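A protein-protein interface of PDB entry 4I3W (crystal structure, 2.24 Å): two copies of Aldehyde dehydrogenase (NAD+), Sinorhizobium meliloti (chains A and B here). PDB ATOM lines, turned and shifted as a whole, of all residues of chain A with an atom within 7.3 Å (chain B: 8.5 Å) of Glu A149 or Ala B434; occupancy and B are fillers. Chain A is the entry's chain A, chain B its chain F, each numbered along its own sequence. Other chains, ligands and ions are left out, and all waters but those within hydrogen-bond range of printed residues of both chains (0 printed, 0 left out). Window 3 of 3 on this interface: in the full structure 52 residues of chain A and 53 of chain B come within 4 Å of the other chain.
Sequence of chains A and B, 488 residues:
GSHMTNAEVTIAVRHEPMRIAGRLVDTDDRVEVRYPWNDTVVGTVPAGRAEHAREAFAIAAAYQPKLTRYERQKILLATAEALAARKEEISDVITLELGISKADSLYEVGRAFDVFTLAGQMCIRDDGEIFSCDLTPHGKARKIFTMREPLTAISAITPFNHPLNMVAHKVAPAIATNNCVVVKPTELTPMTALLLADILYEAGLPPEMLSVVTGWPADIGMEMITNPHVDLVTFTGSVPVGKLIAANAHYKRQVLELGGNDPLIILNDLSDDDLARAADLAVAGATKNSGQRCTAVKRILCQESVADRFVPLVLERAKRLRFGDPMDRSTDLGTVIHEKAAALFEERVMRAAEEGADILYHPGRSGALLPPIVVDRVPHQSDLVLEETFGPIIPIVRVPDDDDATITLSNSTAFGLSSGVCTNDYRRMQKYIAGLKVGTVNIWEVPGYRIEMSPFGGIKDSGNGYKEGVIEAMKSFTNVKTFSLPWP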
ATOM      1  N   MET A 147     -25.900  31.377  27.435  1.00  0.00           N
ATOM      2  CA  MET A 147     -25.907  30.584  26.196  1.00  0.00           C
ATOM      3  C   MET A 147     -25.384  29.194  26.519  1.00  0.00           C
ATOM      4  O   MET A 147     -24.788  28.996  27.587  1.00  0.00           O
ATOM      5  CB  MET A 147     -24.991  31.256  25.162  1.00  0.00           C
ATOM      6  CG  MET A 147     -23.559  31.419  25.655  1.00  0.00           C
ATOM      7  SD  MET A 147     -22.373  32.273  24.549  1.00  0.00           S
ATOM      8  CE  MET A 147     -22.109  31.049  23.272  1.00  0.00           C
ATOM      9  N   ARG A 148     -25.534  28.247  25.595  1.00  0.00           N
ATOM     10  CA  ARG A 148     -25.110  26.886  25.875  1.00  0.00           C
ATOM     11  C   ARG A 148     -24.007  26.459  24.917  1.00  0.00           C
ATOM     12  O   ARG A 148     -23.966  26.908  23.795  1.00  0.00           O
ATOM     13  CB  ARG A 148     -26.293  25.924  25.744  1.00  0.00           C
ATOM     14  CG  ARG A 148     -27.348  26.144  26.789  1.00  0.00           C
ATOM     15  CD  ARG A 148     -28.521  25.211  26.565  1.00  0.00           C
ATOM     16  NE  ARG A 148     -29.493  25.394  27.639  1.00  0.00           N
ATOM     17  CZ  ARG A 148     -29.402  24.835  28.840  1.00  0.00           C
ATOM     18  NH1 ARG A 148     -28.397  24.006  29.121  1.00  0.00           N
ATOM     19  NH2 ARG A 148     -30.346  25.072  29.739  1.00  0.00           N
ATOM     20  N   GLU A 149     -23.120  25.585  25.371  1.00  0.00           N
ATOM     21  CA  GLU A 149     -22.052  25.092  24.535  1.00  0.00           C
ATOM     22  C   GLU A 149     -21.976  23.582  24.767  1.00  0.00           C
ATOM     23  O   GLU A 149     -22.373  23.099  25.824  1.00  0.00           O
ATOM     24  CB  GLU A 149     -20.709  25.758  24.920  1.00  0.00           C
ATOM     25  CG  GLU A 149     -20.689  27.269  24.672  1.00  0.00           C
ATOM     26  CD  GLU A 149     -19.372  27.960  25.104  1.00  0.00           C
ATOM     27  OE1 GLU A 149     -18.637  27.412  25.971  1.00  0.00           O
ATOM     28  OE2 GLU A 149     -19.061  29.075  24.575  1.00  0.00           O
ATOM     29  N   PRO A 150     -21.447  22.842  23.778  1.00  0.00           N
ATOM     30  CA  PRO A 150     -21.386  21.376  23.873  1.00  0.00           C
ATOM     31  C   PRO A 150     -20.233  20.929  24.793  1.00  0.00           C
ATOM     32  O   PRO A 150     -19.409  21.745  25.238  1.00  0.00           O
ATOM     33  CB  PRO A 150     -21.167  20.944  22.413  1.00  0.00           C
ATOM     34  CG  PRO A 150     -20.398  22.123  21.785  1.00  0.00           C
ATOM     35  CD  PRO A 150     -21.055  23.344  22.436  1.00  0.00           C
ATOM     36  N   LEU A 151     -20.217  19.642  25.104  1.00  0.00           N
ATOM     37  CA  LEU A 151     -19.184  19.041  25.917  1.00  0.00           C
ATOM     38  C   LEU A 151     -18.054  18.528  25.015  1.00  0.00           C
ATOM     39  O   LEU A 151     -18.106  18.632  23.767  1.00  0.00           O
ATOM     40  CB  LEU A 151     -19.791  17.873  26.714  1.00  0.00           C
ATOM     41  CG  LEU A 151     -21.074  18.224  27.473  1.00  0.00           C
ATOM     42  CD1 LEU A 151     -21.612  17.035  28.300  1.00  0.00           C
ATOM     43  CD2 LEU A 151     -20.829  19.441  28.402  1.00  0.00           C
ATOM     44  N   THR A 177     -27.204  19.199  19.761  1.00  0.00           N
ATOM     45  CA  THR A 177     -26.437  20.169  20.530  1.00  0.00           C
ATOM     46  C   THR A 177     -24.956  20.238  20.138  1.00  0.00           C
ATOM     47  O   THR A 177     -24.143  20.804  20.876  1.00  0.00           O
ATOM     48  CB  THR A 177     -26.547  19.883  22.049  1.00  0.00           C
ATOM     49  OG1 THR A 177     -26.299  18.499  22.275  1.00  0.00           O
ATOM     50  CG2 THR A 177     -27.957  20.195  22.578  1.00  0.00           C
ATOM     51  N   ASN A 178     -24.605  19.673  18.985  1.00  0.00           N
ATOM     52  CA  ASN A 178     -23.212  19.698  18.517  1.00  0.00           C
ATOM     53  C   ASN A 178     -22.222  18.965  19.419  1.00  0.00           C
ATOM     54  O   ASN A 178     -21.075  19.388  19.618  1.00  0.00           O
ATOM     55  CB  ASN A 178     -22.757  21.142  18.254  1.00  0.00           C
ATOM     56  CG  ASN A 178     -23.011  21.553  16.820  1.00  0.00           C
ATOM     57  OD1 ASN A 178     -23.250  20.680  15.949  1.00  0.00           O
ATOM     58  ND2 ASN A 178     -22.971  22.862  16.548  1.00  0.00           N
ATOM     59  N   ASN A 179     -22.688  17.871  20.002  1.00  0.00           N
ATOM     60  CA  ASN A 179     -21.812  17.014  20.776  1.00  0.00           C
ATOM     61  C   ASN A 179     -21.269  15.882  19.917  1.00  0.00           C
ATOM     62  O   ASN A 179     -21.761  15.645  18.800  1.00  0.00           O
ATOM     63  CB  ASN A 179     -22.573  16.459  21.990  1.00  0.00           C
ATOM     64  CG  ASN A 179     -22.581  17.451  23.142  1.00  0.00           C
ATOM     65  OD1 ASN A 179     -21.540  17.625  23.832  1.00  0.00           O
ATOM     66  ND2 ASN A 179     -23.717  18.151  23.335  1.00  0.00           N
ATOM     67  N   ARG A 253     -20.182  14.015  34.885  1.00  0.00           N
ATOM     68  CA  ARG A 253     -21.640  14.019  35.013  1.00  0.00           C
ATOM     69  C   ARG A 253     -22.183  12.656  34.603  1.00  0.00           C
ATOM     70  O   ARG A 253     -21.609  11.992  33.732  1.00  0.00           O
ATOM     71  CB  ARG A 253     -22.251  15.074  34.138  1.00  0.00           C
ATOM     72  CG  ARG A 253     -21.353  16.254  34.004  1.00  0.00           C
ATOM     73  CD  ARG A 253     -22.053  17.510  34.414  1.00  0.00           C
ATOM     74  NE  ARG A 253     -22.811  18.093  33.307  1.00  0.00           N
ATOM     75  CZ  ARG A 253     -22.278  18.877  32.365  1.00  0.00           C
ATOM     76  NH1 ARG A 253     -20.963  19.156  32.369  1.00  0.00           N
ATOM     77  NH2 ARG A 253     -23.068  19.382  31.417  1.00  0.00           N
ATOM     78  N   MET A 474     -31.090  17.424  25.949  1.00  0.00           N
ATOM     79  CA  MET A 474     -30.382  18.546  25.300  1.00  0.00           C
ATOM     80  C   MET A 474     -29.767  19.548  26.283  1.00  0.00           C
ATOM     81  O   MET A 474     -28.636  20.003  26.069  1.00  0.00           O
ATOM     82  CB  MET A 474     -31.265  19.277  24.279  1.00  0.00           C
ATOM     83  CG  MET A 474     -31.517  18.442  23.051  1.00  0.00           C
ATOM     84  SD  MET A 474     -32.723  19.095  21.888  1.00  0.00           S
ATOM     85  CE  MET A 474     -31.877  20.619  21.379  1.00  0.00           C
ATOM     86  N   LYS A 475     -30.499  19.920  27.337  1.00  0.00           N
ATOM     87  CA  LYS A 475     -29.917  20.809  28.359  1.00  0.00           C
ATOM     88  C   LYS A 475     -28.749  20.153  29.069  1.00  0.00           C
ATOM     89  O   LYS A 475     -27.701  20.770  29.345  1.00  0.00           O
ATOM     90  CB  LYS A 475     -30.962  21.187  29.391  1.00  0.00           C
ATOM     91  CG  LYS A 475     -32.174  21.954  28.828  1.00  0.00           C
ATOM     92  CD  LYS A 475     -33.045  22.411  30.022  1.00  0.00           C
ATOM     93  CE  LYS A 475     -34.485  22.663  29.650  1.00  0.00           C
ATOM     94  NZ  LYS A 475     -35.314  22.748  30.909  1.00  0.00           N
ATOM     95  N   PHE A 477     -26.719  17.856  28.022  1.00  0.00           N
ATOM     96  CA  PHE A 477     -25.566  17.614  27.180  1.00  0.00           C
ATOM     97  C   PHE A 477     -24.828  18.928  26.858  1.00  0.00           C
ATOM     98  O   PHE A 477     -23.977  18.969  25.967  1.00  0.00           O
ATOM     99  CB  PHE A 477     -26.015  16.958  25.870  1.00  0.00           C
ATOM    100  CG  PHE A 477     -26.522  15.541  26.023  1.00  0.00           C
ATOM    101  CD1 PHE A 477     -26.529  14.907  27.255  1.00  0.00           C
ATOM    102  CD2 PHE A 477     -26.974  14.838  24.904  1.00  0.00           C
ATOM    103  CE1 PHE A 477     -26.979  13.592  27.379  1.00  0.00           C
ATOM    104  CE2 PHE A 477     -27.432  13.512  25.016  1.00  0.00           C
ATOM    105  CZ  PHE A 477     -27.439  12.902  26.266  1.00  0.00           C
ATOM    106  N   THR A 478     -25.154  20.005  27.564  1.00  0.00           N
ATOM    107  CA  THR A 478     -24.448  21.256  27.346  1.00  0.00           C
ATOM    108  C   THR A 478     -23.926  21.870  28.635  1.00  0.00           C
ATOM    109  O   THR A 478     -24.335  21.486  29.730  1.00  0.00           O
ATOM    110  CB  THR A 478     -25.364  22.304  26.671  1.00  0.00           C
ATOM    111  OG1 THR A 478     -26.481  22.578  27.531  1.00  0.00           O
ATOM    112  CG2 THR A 478     -25.885  21.786  25.348  1.00  0.00           C
ATOM    113  N   ASN A 479     -23.049  22.861  28.488  1.00  0.00           N
ATOM    114  CA  ASN A 479     -22.676  23.720  29.609  1.00  0.00           C
ATOM    115  C   ASN A 479     -23.288  25.084  29.383  1.00  0.00           C
ATOM    116  O   ASN A 479     -23.293  25.618  28.248  1.00  0.00           O
ATOM    117  CB  ASN A 479     -21.154  23.910  29.707  1.00  0.00           C
ATOM    118  CG  ASN A 479     -20.463  22.691  30.178  1.00  0.00           C
ATOM    119  OD1 ASN A 479     -20.919  22.019  31.122  1.00  0.00           O
ATOM    120  ND2 ASN A 479     -19.352  22.362  29.513  1.00  0.00           N
ATOM    121  N   VAL A 480     -23.817  25.663  30.445  1.00  0.00           N
ATOM    122  CA  VAL A 480     -24.310  27.025  30.340  1.00  0.00           C
ATOM    123  C   VAL A 480     -23.151  27.996  30.572  1.00  0.00           C
ATOM    124  O   VAL A 480     -22.440  27.917  31.576  1.00  0.00           O
ATOM    125  CB  VAL A 480     -25.434  27.276  31.372  1.00  0.00           C
ATOM    126  CG1 VAL A 480     -25.763  28.772  31.447  1.00  0.00           C
ATOM    127  CG2 VAL A 480     -26.702  26.401  31.025  1.00  0.00           C
ATOM    128  N   LYS A 481     -22.935  28.898  29.627  1.00  0.00           N
ATOM    129  CA  LYS A 481     -21.968  29.962  29.862  1.00  0.00           C
ATOM    130  C   LYS A 481     -22.754  31.269  30.036  1.00  0.00           C
ATOM    131  O   LYS A 481     -23.691  31.529  29.290  1.00  0.00           O
ATOM    132  CB  LYS A 481     -20.999  30.068  28.653  1.00  0.00           C
ATOM    133  CG  LYS A 481     -20.049  31.290  28.717  1.00  0.00           C
ATOM    134  CD  LYS A 481     -19.153  31.421  27.466  1.00  0.00           C
ATOM    135  CE  LYS A 481     -17.995  30.446  27.512  1.00  0.00           C
ATOM    136  NZ  LYS A 481     -17.098  30.518  26.345  1.00  0.00           N
ATOM    137  N   PHE A 483     -22.512  35.649  30.260  1.00  0.00           N
ATOM    138  CA  PHE A 483     -21.623  36.791  29.959  1.00  0.00           C
ATOM    139  C   PHE A 483     -22.375  38.026  30.338  1.00  0.00           C
ATOM    140  O   PHE A 483     -23.602  38.083  30.241  1.00  0.00           O
ATOM    141  CB  PHE A 483     -21.094  36.824  28.487  1.00  0.00           C
ATOM    142  CG  PHE A 483     -22.175  36.954  27.422  1.00  0.00           C
ATOM    143  CD1 PHE A 483     -22.808  35.821  26.914  1.00  0.00           C
ATOM    144  CD2 PHE A 483     -22.510  38.197  26.890  1.00  0.00           C
ATOM    145  CE1 PHE A 483     -23.769  35.920  25.925  1.00  0.00           C
ATOM    146  CE2 PHE A 483     -23.488  38.302  25.892  1.00  0.00           C
ATOM    147  CZ  PHE A 483     -24.098  37.147  25.410  1.00  0.00           C
ATOM    148  N   ILE B 407      -6.097  34.290  24.299  1.00  0.00           N
ATOM    149  CA  ILE B 407      -7.157  33.379  24.690  1.00  0.00           C
ATOM    150  C   ILE B 407      -6.567  32.011  25.028  1.00  0.00           C
ATOM    151  O   ILE B 407      -6.910  31.394  26.057  1.00  0.00           O
ATOM    152  CB  ILE B 407      -8.254  33.265  23.588  1.00  0.00           C
ATOM    153  CG1 ILE B 407      -9.078  34.562  23.537  1.00  0.00           C
ATOM    154  CG2 ILE B 407      -9.117  32.032  23.848  1.00  0.00           C
ATOM    155  CD1 ILE B 407     -10.023  34.676  22.316  1.00  0.00           C
ATOM    156  N   ASN B 411      -6.843  30.224  28.706  1.00  0.00           N
ATOM    157  CA  ASN B 411      -7.381  28.866  28.851  1.00  0.00           C
ATOM    158  C   ASN B 411      -6.382  27.779  29.233  1.00  0.00           C
ATOM    159  O   ASN B 411      -6.735  26.585  29.299  1.00  0.00           O
ATOM    160  CB  ASN B 411      -8.080  28.415  27.545  1.00  0.00           C
ATOM    161  CG  ASN B 411      -9.300  29.221  27.232  1.00  0.00           C
ATOM    162  OD1 ASN B 411      -9.911  29.795  28.120  1.00  0.00           O
ATOM    163  ND2 ASN B 411      -9.680  29.253  25.959  1.00  0.00           N
ATOM    164  N   ARG B 427     -16.255  43.610  18.579  1.00  0.00           N
ATOM    165  CA  ARG B 427     -15.848  42.398  17.882  1.00  0.00           C
ATOM    166  C   ARG B 427     -14.943  41.545  18.765  1.00  0.00           C
ATOM    167  O   ARG B 427     -15.020  40.310  18.773  1.00  0.00           O
ATOM    168  CB  ARG B 427     -15.154  42.765  16.568  1.00  0.00           C
ATOM    169  CG  ARG B 427     -14.699  41.583  15.745  1.00  0.00           C
ATOM    170  CD  ARG B 427     -13.611  41.965  14.702  1.00  0.00           C
ATOM    171  NE  ARG B 427     -12.265  41.520  15.097  1.00  0.00           N
ATOM    172  CZ  ARG B 427     -11.302  42.317  15.575  1.00  0.00           C
ATOM    173  NH1 ARG B 427     -11.508  43.622  15.727  1.00  0.00           N
ATOM    174  NH2 ARG B 427     -10.114  41.813  15.902  1.00  0.00           N
ATOM    175  N   ARG B 428     -14.063  42.205  19.504  1.00  0.00           N
ATOM    176  CA  ARG B 428     -13.144  41.490  20.388  1.00  0.00           C
ATOM    177  C   ARG B 428     -13.888  40.976  21.632  1.00  0.00           C
ATOM    178  O   ARG B 428     -13.679  39.835  22.072  1.00  0.00           O
ATOM    179  CB  ARG B 428     -11.990  42.415  20.789  1.00  0.00           C
ATOM    180  CG  ARG B 428     -11.248  42.971  19.581  1.00  0.00           C
ATOM    181  CD  ARG B 428      -9.786  42.792  19.817  1.00  0.00           C
ATOM    182  NE  ARG B 428      -9.179  44.042  20.170  1.00  0.00           N
ATOM    183  CZ  ARG B 428      -7.977  44.177  20.721  1.00  0.00           C
ATOM    184  NH1 ARG B 428      -7.259  43.120  21.062  1.00  0.00           N
ATOM    185  NH2 ARG B 428      -7.510  45.395  20.962  1.00  0.00           N
ATOM    186  N   MET B 429     -14.749  41.813  22.198  1.00  0.00           N
ATOM    187  CA  MET B 429     -15.621  41.350  23.274  1.00  0.00           C
ATOM    188  C   MET B 429     -16.244  39.980  22.937  1.00  0.00           C
ATOM    189  O   MET B 429     -16.151  39.001  23.714  1.00  0.00           O
ATOM    190  CB  MET B 429     -16.768  42.338  23.450  1.00  0.00           C
ATOM    191  CG  MET B 429     -16.616  43.255  24.575  1.00  0.00           C
ATOM    192  SD  MET B 429     -17.954  44.441  24.470  1.00  0.00           S
ATOM    193  CE  MET B 429     -17.002  45.908  24.963  1.00  0.00           C
ATOM    194  N   GLN B 430     -16.888  39.894  21.777  1.00  0.00           N
ATOM    195  CA  GLN B 430     -17.656  38.705  21.538  1.00  0.00           C
ATOM    196  C   GLN B 430     -16.715  37.564  21.239  1.00  0.00           C
ATOM    197  O   GLN B 430     -17.016  36.393  21.523  1.00  0.00           O
ATOM    198  CB  GLN B 430     -18.785  38.910  20.492  1.00  0.00           C
ATOM    199  CG  GLN B 430     -18.525  38.408  19.103  1.00  0.00           C
ATOM    200  CD  GLN B 430     -18.541  36.884  18.940  1.00  0.00           C
ATOM    201  OE1 GLN B 430     -19.384  36.180  19.442  1.00  0.00           O
ATOM    202  NE2 GLN B 430     -17.615  36.395  18.180  1.00  0.00           N
ATOM    203  N   LYS B 431     -15.531  37.881  20.728  1.00  0.00           N
ATOM    204  CA  LYS B 431     -14.541  36.813  20.487  1.00  0.00           C
ATOM    205  C   LYS B 431     -14.086  36.202  21.823  1.00  0.00           C
ATOM    206  O   LYS B 431     -13.951  34.981  21.925  1.00  0.00           O
ATOM    207  CB  LYS B 431     -13.346  37.356  19.729  1.00  0.00           C
ATOM    208  CG  LYS B 431     -12.248  36.344  19.461  1.00  0.00           C
ATOM    209  CD  LYS B 431     -11.138  37.059  18.621  1.00  0.00           C
ATOM    210  CE  LYS B 431      -9.882  36.213  18.429  1.00  0.00           C
ATOM    211  NZ  LYS B 431     -10.133  35.122  17.464  1.00  0.00           N
ATOM    212  N   TYR B 432     -13.841  37.048  22.838  1.00  0.00           N
ATOM    213  CA  TYR B 432     -13.495  36.546  24.176  1.00  0.00           C
ATOM    214  C   TYR B 432     -14.665  35.807  24.841  1.00  0.00           C
ATOM    215  O   TYR B 432     -14.477  34.750  25.439  1.00  0.00           O
ATOM    216  CB  TYR B 432     -12.950  37.652  25.083  1.00  0.00           C
ATOM    217  CG  TYR B 432     -11.508  37.981  24.769  1.00  0.00           C
ATOM    218  CD1 TYR B 432     -11.166  38.778  23.653  1.00  0.00           C
ATOM    219  CD2 TYR B 432     -10.488  37.447  25.532  1.00  0.00           C
ATOM    220  CE1 TYR B 432      -9.827  39.047  23.330  1.00  0.00           C
ATOM    221  CE2 TYR B 432      -9.147  37.719  25.242  1.00  0.00           C
ATOM    222  CZ  TYR B 432      -8.822  38.526  24.141  1.00  0.00           C
ATOM    223  OH  TYR B 432      -7.491  38.782  23.873  1.00  0.00           O
ATOM    224  N   ILE B 433     -15.861  36.364  24.714  1.00  0.00           N
ATOM    225  CA  ILE B 433     -17.037  35.729  25.267  1.00  0.00           C
ATOM    226  C   ILE B 433     -17.150  34.321  24.698  1.00  0.00           C
ATOM    227  O   ILE B 433     -17.348  33.360  25.431  1.00  0.00           O
ATOM    228  CB  ILE B 433     -18.314  36.584  25.021  1.00  0.00           C
ATOM    229  CG1 ILE B 433     -18.270  37.826  25.913  1.00  0.00           C
ATOM    230  CG2 ILE B 433     -19.582  35.739  25.266  1.00  0.00           C
ATOM    231  CD1 ILE B 433     -19.169  38.967  25.472  1.00  0.00           C
ATOM    232  N   ALA B 434     -16.934  34.174  23.395  1.00  0.00           N
ATOM    233  CA  ALA B 434     -17.093  32.857  22.792  1.00  0.00           C
ATOM    234  C   ALA B 434     -15.919  31.930  23.078  1.00  0.00           C
ATOM    235  O   ALA B 434     -16.085  30.690  23.170  1.00  0.00           O
ATOM    236  CB  ALA B 434     -17.305  32.955  21.296  1.00  0.00           C
ATOM    237  N   GLY B 435     -14.724  32.503  23.171  1.00  0.00           N
ATOM    238  CA  GLY B 435     -13.505  31.690  23.238  1.00  0.00           C
ATOM    239  C   GLY B 435     -12.954  31.312  24.624  1.00  0.00           C
ATOM    240  O   GLY B 435     -12.214  30.319  24.754  1.00  0.00           O
ATOM    241  N   LEU B 436     -13.273  32.084  25.667  1.00  0.00           N
ATOM    242  CA  LEU B 436     -12.733  31.718  26.979  1.00  0.00           C
ATOM    243  C   LEU B 436     -13.467  30.501  27.481  1.00  0.00           C
ATOM    244  O   LEU B 436     -14.722  30.440  27.424  1.00  0.00           O
ATOM    245  CB  LEU B 436     -12.840  32.851  27.992  1.00  0.00           C
ATOM    246  CG  LEU B 436     -12.039  34.092  27.607  1.00  0.00           C
ATOM    247  CD1 LEU B 436     -12.369  35.287  28.543  1.00  0.00           C
ATOM    248  CD2 LEU B 436     -10.573  33.681  27.639  1.00  0.00           C
ATOM    249  N   LYS B 437     -12.705  29.519  27.975  1.00  0.00           N
ATOM    250  CA  LYS B 437     -13.334  28.306  28.520  1.00  0.00           C
ATOM    251  C   LYS B 437     -13.657  28.413  29.994  1.00  0.00           C
ATOM    252  O   LYS B 437     -12.929  27.887  30.855  1.00  0.00           O
ATOM    253  CB  LYS B 437     -12.447  27.105  28.239  1.00  0.00           C
ATOM    254  CG  LYS B 437     -12.676  26.594  26.818  1.00  0.00           C
ATOM    255  CD  LYS B 437     -11.440  26.649  25.981  1.00  0.00           C
ATOM    256  CE  LYS B 437     -11.098  25.269  25.446  1.00  0.00           C
ATOM    257  NZ  LYS B 437     -10.567  25.356  24.064  1.00  0.00           N
ATOM    258  N   VAL B 438     -14.764  29.093  30.280  1.00  0.00           N
ATOM    259  CA  VAL B 438     -15.130  29.439  31.646  1.00  0.00           C
ATOM    260  C   VAL B 438     -16.654  29.376  31.764  1.00  0.00           C
ATOM    261  O   VAL B 438     -17.339  29.242  30.746  1.00  0.00           O
ATOM    262  CB  VAL B 438     -14.655  30.879  31.963  1.00  0.00           C
ATOM    263  CG1 VAL B 438     -13.127  30.924  31.984  1.00  0.00           C
ATOM    264  CG2 VAL B 438     -15.204  31.871  30.901  1.00  0.00           C
ATOM    265  N   GLY B 439     -17.181  29.466  32.989  1.00  0.00           N
ATOM    266  CA  GLY B 439     -18.611  29.597  33.174  1.00  0.00           C
ATOM    267  C   GLY B 439     -19.169  31.008  32.961  1.00  0.00           C
ATOM    268  O   GLY B 439     -20.353  31.155  32.651  1.00  0.00           O
ATOM    269  N   VAL B 441     -18.103  35.238  31.619  1.00  0.00           N
ATOM    270  CA  VAL B 441     -17.215  36.270  31.097  1.00  0.00           C
ATOM    271  C   VAL B 441     -17.824  37.632  31.352  1.00  0.00           C
ATOM    272  O   VAL B 441     -18.865  37.956  30.768  1.00  0.00           O
ATOM    273  CB  VAL B 441     -17.028  36.123  29.567  1.00  0.00           C
ATOM    274  CG1 VAL B 441     -16.067  37.205  29.015  1.00  0.00           C
ATOM    275  CG2 VAL B 441     -16.517  34.735  29.230  1.00  0.00           C
ATOM    276  N   ILE B 443     -17.713  41.638  30.935  1.00  0.00           N
ATOM    277  CA  ILE B 443     -17.057  42.700  30.180  1.00  0.00           C
ATOM    278  C   ILE B 443     -16.960  43.942  31.063  1.00  0.00           C
ATOM    279  O   ILE B 443     -17.981  44.445  31.569  1.00  0.00           O
ATOM    280  CB  ILE B 443     -17.787  43.032  28.870  1.00  0.00           C
ATOM    281  CG1 ILE B 443     -17.849  41.815  27.965  1.00  0.00           C
ATOM    282  CG2 ILE B 443     -17.086  44.186  28.124  1.00  0.00           C
ATOM    283  CD1 ILE B 443     -16.473  41.211  27.619  1.00  0.00           C
ATOM    284  N   ILE B 459     -16.269  24.977  34.868  1.00  0.00           N
ATOM    285  CA  ILE B 459     -16.031  23.719  34.178  1.00  0.00           C
ATOM    286  C   ILE B 459     -14.584  23.299  34.494  1.00  0.00           C
ATOM    287  O   ILE B 459     -13.922  23.924  35.345  1.00  0.00           O
ATOM    288  CB  ILE B 459     -16.233  23.920  32.699  1.00  0.00           C
ATOM    289  CG1 ILE B 459     -15.369  25.093  32.230  1.00  0.00           C
ATOM    290  CG2 ILE B 459     -17.696  24.257  32.420  1.00  0.00           C
ATOM    291  CD1 ILE B 459     -15.280  25.188  30.717  1.00  0.00           C
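The side-chain amino group (NZ) of Lys A481 sits at hydrogen-bond distance from the backbone carbonyl oxygen (O) of Ile B433, 3.0 Å away. The side-chain amino group (NZ) of Lys A481 lies within hydrogen-bond range of the backbone carbonyl oxygen (O) of Ala B434 (3.3 Å). The side-chain amino group of Lys A481 is in hydrogen-bond range of the backbone carbonyl oxygen of Leu B436 (2.6 Å).
The backbone carbonyl oxygen (O) of Met A147 sits at hydrogen-bond distance from the backbone NH (N) of Lys A481 (2.8 Å). The backbone carbonyl oxygen of Glu A149 lies within hydrogen-bond range of the backbone NH of Asn A479. The side-chain carboxylate of Glu A149 lies within salt-bridge range of the side-chain amino group of Lys A481. The side-chain amide oxygen (OD1) of Asn A479 is in hydrogen-bond range of the guanidinium group (NH1) of Arg A253, 3.1 Å away.
Ala B434 touches Glu A149. Asn A479 touches Ile B459. O of Val A480 touches O of Gly B439 (3.999 Å). Val B438 touches Lys A481 (O to CE, 3.5 Å). Lys A481 touches Gly B439. Phe A483 touches Ile B433. Val B441 touches Phe A483.
Of chain B, only Ala B434 (3.7 Å) comes within 4 Å of Glu A149. No residue of chain B comes within 4 Å of Pro A150. Of the printed residues of chain B, Val A480 touches Gly B439. Printed residues of chain B within 4 Å of Phe A483: Ile B433 and Val B441. Asn B411 touches none of the printed residues of chain A. Gln B430 touches none of the printed residues of chain A. Ala B434 touches just these residues of chain A: Glu A149 (3.7 Å) and Lys A481 (3.3 Å). Of the printed residues of chain A, Leu B436 touches Lys A481. Of the printed residues of chain A, Val B438 touches Lys A481. Printed residues of chain A within 4 Å of Gly B439: Val A480 (3.999 Å) and Lys A481 (3.4 Å). The nearest residue of chain B that does not touch Glu A149 is Ile B433 (4.7 Å). The nearest residue of chain A that does not touch Ala B434 is Met A147 (5.4 Å). The nearest printed residue of chain A that does not touch Gly B439 is Phe A483 (5.5 Å).
Hydrophobic or aromatic side chains of chain A within 4 Å of the printed part of chain B: Phe A483. Of the 18 printed residues of chain B, 7 touch a printed residue of chain A. Among the printed residues, no Asp or Glu carboxylate lies within 4 Å of a Lys or Arg side-chain nitrogen of the other chain.
No position is printed for both chains. Of the 10 pairs that touch across the chains among the printed residues, none has its exchanged pair printed and touching as well.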
